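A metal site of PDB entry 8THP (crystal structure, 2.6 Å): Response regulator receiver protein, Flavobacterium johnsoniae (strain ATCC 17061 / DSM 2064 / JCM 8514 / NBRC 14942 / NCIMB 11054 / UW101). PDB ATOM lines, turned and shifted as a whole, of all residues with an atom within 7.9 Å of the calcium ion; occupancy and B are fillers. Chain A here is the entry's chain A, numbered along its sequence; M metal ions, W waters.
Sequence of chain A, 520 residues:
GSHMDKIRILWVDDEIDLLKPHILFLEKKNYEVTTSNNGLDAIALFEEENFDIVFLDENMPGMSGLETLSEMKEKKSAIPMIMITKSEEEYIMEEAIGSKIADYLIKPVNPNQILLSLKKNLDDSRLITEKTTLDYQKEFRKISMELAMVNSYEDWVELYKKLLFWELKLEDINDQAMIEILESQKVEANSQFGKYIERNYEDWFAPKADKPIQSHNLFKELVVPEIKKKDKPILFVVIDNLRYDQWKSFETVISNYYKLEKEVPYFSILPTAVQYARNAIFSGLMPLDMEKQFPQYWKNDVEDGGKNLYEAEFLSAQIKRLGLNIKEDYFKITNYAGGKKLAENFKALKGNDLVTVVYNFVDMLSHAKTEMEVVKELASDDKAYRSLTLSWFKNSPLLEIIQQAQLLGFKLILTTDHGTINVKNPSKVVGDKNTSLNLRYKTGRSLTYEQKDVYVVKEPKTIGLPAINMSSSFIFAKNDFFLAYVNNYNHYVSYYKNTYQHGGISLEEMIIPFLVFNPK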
ATOM      1  N   VAL A  12      30.846  22.070  11.352  1.00  0.00           N
ATOM      2  CA  VAL A  12      31.007  23.020  10.271  1.00  0.00           C
ATOM      3  C   VAL A  12      30.534  24.405  10.730  1.00  0.00           C
ATOM      4  O   VAL A  12      29.362  24.587  11.090  1.00  0.00           O
ATOM      5  CB  VAL A  12      30.195  22.572   9.037  1.00  0.00           C
ATOM      6  CG1 VAL A  12      30.674  23.264   7.760  1.00  0.00           C
ATOM      7  CG2 VAL A  12      30.213  21.061   8.864  1.00  0.00           C
ATOM      8  N   ASP A  13      31.441  25.389  10.716  1.00  0.00           N
ATOM      9  CA  ASP A  13      31.096  26.770  11.048  1.00  0.00           C
ATOM     10  C   ASP A  13      32.108  27.703  10.364  1.00  0.00           C
ATOM     11  O   ASP A  13      33.281  27.373  10.309  1.00  0.00           O
ATOM     12  CB  ASP A  13      31.074  26.998  12.565  1.00  0.00           C
ATOM     13  CG  ASP A  13      30.356  28.264  13.004  1.00  0.00           C
ATOM     14  OD1 ASP A  13      30.803  29.367  12.601  1.00  0.00           O
ATOM     15  OD2 ASP A  13      29.355  28.136  13.760  1.00  0.00           O
ATOM     16  N   ASP A  14      31.622  28.855   9.868  1.00  0.00           N
ATOM     17  CA  ASP A  14      32.495  29.872   9.273  1.00  0.00           C
ATOM     18  C   ASP A  14      33.417  30.432  10.345  1.00  0.00           C
ATOM     19  O   ASP A  14      34.619  30.591  10.083  1.00  0.00           O
ATOM     20  CB  ASP A  14      31.735  30.994   8.561  1.00  0.00           C
ATOM     21  CG  ASP A  14      30.642  31.632   9.408  1.00  0.00           C
ATOM     22  OD1 ASP A  14      29.730  30.912   9.815  1.00  0.00           O
ATOM     23  OD2 ASP A  14      30.705  32.854   9.642  1.00  0.00           O
ATOM     24  N   GLU A  15      32.884  30.635  11.563  1.00  0.00           N
ATOM     25  CA  GLU A  15      33.640  31.197  12.682  1.00  0.00           C
ATOM     26  C   GLU A  15      34.114  30.065  13.593  1.00  0.00           C
ATOM     27  O   GLU A  15      33.865  30.088  14.793  1.00  0.00           O
ATOM     28  CB  GLU A  15      32.765  32.179  13.457  1.00  0.00           C
ATOM     29  CG  GLU A  15      32.284  33.379  12.654  1.00  0.00           C
ATOM     30  CD  GLU A  15      31.120  34.147  13.286  1.00  0.00           C
ATOM     31  OE1 GLU A  15      30.630  33.719  14.337  1.00  0.00           O
ATOM     32  OE2 GLU A  15      30.700  35.166  12.715  1.00  0.00           O
ATOM     33  N   ILE A  16      34.782  29.052  13.026  1.00  0.00           N
ATOM     34  CA  ILE A  16      35.119  27.850  13.786  1.00  0.00           C
ATOM     35  C   ILE A  16      36.269  28.095  14.768  1.00  0.00           C
ATOM     36  O   ILE A  16      36.595  27.230  15.584  1.00  0.00           O
ATOM     37  CB  ILE A  16      35.405  26.660  12.834  1.00  0.00           C
ATOM     38  CG1 ILE A  16      35.106  25.298  13.470  1.00  0.00           C
ATOM     39  CG2 ILE A  16      36.813  26.740  12.278  1.00  0.00           C
ATOM     40  CD1 ILE A  16      33.649  25.089  13.850  1.00  0.00           C
ATOM     41  N   ASP A  57      26.446  25.080  11.311  1.00  0.00           N
ATOM     42  CA  ASP A  57      25.960  26.451  11.382  1.00  0.00           C
ATOM     43  C   ASP A  57      25.044  26.697  10.185  1.00  0.00           C
ATOM     44  O   ASP A  57      25.292  26.126   9.138  1.00  0.00           O
ATOM     45  CB  ASP A  57      27.132  27.444  11.400  1.00  0.00           C
ATOM     46  CG  ASP A  57      26.748  28.881  11.644  1.00  0.00           C
ATOM     47  OD1 ASP A  57      25.567  29.166  11.903  1.00  0.00           O
ATOM     48  OD2 ASP A  57      27.639  29.724  11.551  1.00  0.00           O
ATOM     49  N   GLU A  58      24.042  27.567  10.324  1.00  0.00           N
ATOM     50  CA  GLU A  58      23.211  27.973   9.197  1.00  0.00           C
ATOM     51  C   GLU A  58      23.907  29.080   8.393  1.00  0.00           C
ATOM     52  O   GLU A  58      24.359  28.830   7.286  1.00  0.00           O
ATOM     53  CB  GLU A  58      21.811  28.396   9.642  1.00  0.00           C
ATOM     54  CG  GLU A  58      21.013  29.141   8.584  1.00  0.00           C
ATOM     55  CD  GLU A  58      20.700  28.385   7.313  1.00  0.00           C
ATOM     56  OE1 GLU A  58      21.005  27.168   7.243  1.00  0.00           O
ATOM     57  OE2 GLU A  58      20.103  28.995   6.407  1.00  0.00           O
ATOM     58  N   ASN A  59      23.965  30.311   8.926  1.00  0.00           N
ATOM     59  CA  ASN A  59      24.480  31.448   8.168  1.00  0.00           C
ATOM     60  C   ASN A  59      25.973  31.273   7.989  1.00  0.00           C
ATOM     61  O   ASN A  59      26.723  31.455   8.946  1.00  0.00           O
ATOM     62  CB  ASN A  59      24.170  32.785   8.849  1.00  0.00           C
ATOM     63  CG  ASN A  59      22.842  33.366   8.403  1.00  0.00           C
ATOM     64  OD1 ASN A  59      22.696  33.707   7.233  1.00  0.00           O
ATOM     65  ND2 ASN A  59      21.885  33.501   9.309  1.00  0.00           N
ATOM     66  N   MET A  60      26.356  30.854   6.776  1.00  0.00           N
ATOM     67  CA  MET A  60      27.738  30.562   6.439  1.00  0.00           C
ATOM     68  C   MET A  60      28.036  31.129   5.050  1.00  0.00           C
ATOM     69  O   MET A  60      27.256  30.922   4.125  1.00  0.00           O
ATOM     70  CB  MET A  60      28.004  29.050   6.442  1.00  0.00           C
ATOM     71  CG  MET A  60      28.576  28.528   7.755  1.00  0.00           C
ATOM     72  SD  MET A  60      28.988  26.749   7.708  1.00  0.00           S
ATOM     73  CE  MET A  60      27.712  26.082   6.651  1.00  0.00           C
ATOM     74  N   PRO A  61      29.154  31.860   4.869  1.00  0.00           N
ATOM     75  CA  PRO A  61      29.621  32.210   3.528  1.00  0.00           C
ATOM     76  C   PRO A  61      29.789  30.926   2.715  1.00  0.00           C
ATOM     77  O   PRO A  61      30.545  30.040   3.125  1.00  0.00           O
ATOM     78  CB  PRO A  61      30.992  32.874   3.771  1.00  0.00           C
ATOM     79  CG  PRO A  61      30.916  33.372   5.202  1.00  0.00           C
ATOM     80  CD  PRO A  61      30.028  32.380   5.928  1.00  0.00           C
ATOM     81  N   ILE A  84      23.760  24.231  15.184  1.00  0.00           N
ATOM     82  CA  ILE A  84      24.200  25.186  16.196  1.00  0.00           C
ATOM     83  C   ILE A  84      24.433  26.541  15.538  1.00  0.00           C
ATOM     84  O   ILE A  84      25.405  26.703  14.819  1.00  0.00           O
ATOM     85  CB  ILE A  84      25.504  24.698  16.880  1.00  0.00           C
ATOM     86  CG1 ILE A  84      25.411  23.227  17.293  1.00  0.00           C
ATOM     87  CG2 ILE A  84      25.887  25.602  18.057  1.00  0.00           C
ATOM     88  CD1 ILE A  84      26.632  22.719  18.005  1.00  0.00           C
ATOM     89  N   THR A  85      23.577  27.523  15.805  1.00  0.00           N
ATOM     90  CA  THR A  85      23.615  28.801  15.104  1.00  0.00           C
ATOM     91  C   THR A  85      22.885  29.878  15.901  1.00  0.00           C
ATOM     92  O   THR A  85      22.190  29.569  16.867  1.00  0.00           O
ATOM     93  CB  THR A  85      22.971  28.693  13.706  1.00  0.00           C
ATOM     94  OG1 THR A  85      23.004  29.978  13.077  1.00  0.00           O
ATOM     95  CG2 THR A  85      21.538  28.197  13.721  1.00  0.00           C
ATOM     96  N   LYS A  86      23.006  31.141  15.461  1.00  0.00           N
ATOM     97  CA  LYS A  86      22.382  32.281  16.125  1.00  0.00           C
ATOM     98  C   LYS A  86      20.956  32.483  15.616  1.00  0.00           C
ATOM     99  O   LYS A  86      20.178  33.179  16.251  1.00  0.00           O
ATOM    100  CB  LYS A  86      23.203  33.551  15.891  1.00  0.00           C
ATOM    101  CG  LYS A  86      24.576  33.581  16.560  1.00  0.00           C
ATOM    102  CD  LYS A  86      25.207  34.968  16.669  1.00  0.00           C
ATOM    103  CE  LYS A  86      26.474  35.003  17.512  1.00  0.00           C
ATOM    104  NZ  LYS A  86      26.247  34.634  18.938  1.00  0.00           N
ATOM    105  N   LYS A 107      22.720  29.979  19.477  1.00  0.00           N
ATOM    106  CA  LYS A 107      23.909  30.588  20.072  1.00  0.00           C
ATOM    107  C   LYS A 107      23.495  31.850  20.835  1.00  0.00           C
ATOM    108  O   LYS A 107      22.389  32.375  20.637  1.00  0.00           O
ATOM    109  CB  LYS A 107      24.918  30.972  18.986  1.00  0.00           C
ATOM    110  CG  LYS A 107      25.620  29.829  18.292  1.00  0.00           C
ATOM    111  CD  LYS A 107      26.572  30.311  17.211  1.00  0.00           C
ATOM    112  CE  LYS A 107      27.262  29.209  16.448  1.00  0.00           C
ATOM    113  NZ  LYS A 107      27.904  29.734  15.220  1.00  0.00           N
HETATM  114 CA    CA M   1      28.188  31.960  10.811  1.00  0.00          CA
HETATM  115  O   HOH W   1      26.405  33.839  11.884  1.00  0.00           O
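OD2 of Asp 57 sits close to NZ of Lys 107, 3.7 Å away. The side-chain carboxylate of Asp 57 lies within hydrogen-bond range of the side-chain hydroxyl of Thr 85 (2.9 Å). The backbone NH (N) of Asp 57 lies within hydrogen-bond range of the backbone carbonyl oxygen (O) of Val 12, 3.0 Å away.
Of the 14 residues printed, 3 come within 4 Å of the calcium ion. The nearest printed residue that does not touch the calcium ion is Asp 13 (4.1 Å).
The side-chain carboxylate (OD1) of Asp 14 binds the calcium ion. The calcium ion is bound by OD2 of Asp 57 (2.4 Å). O of Asn 59 is bound to the calcium ion (2.4 Å). The calcium ion is bound by water W1 (2.8 Å). Slightly farther from the calcium ion lies OD2 of Asp 14 (2.9 Å).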
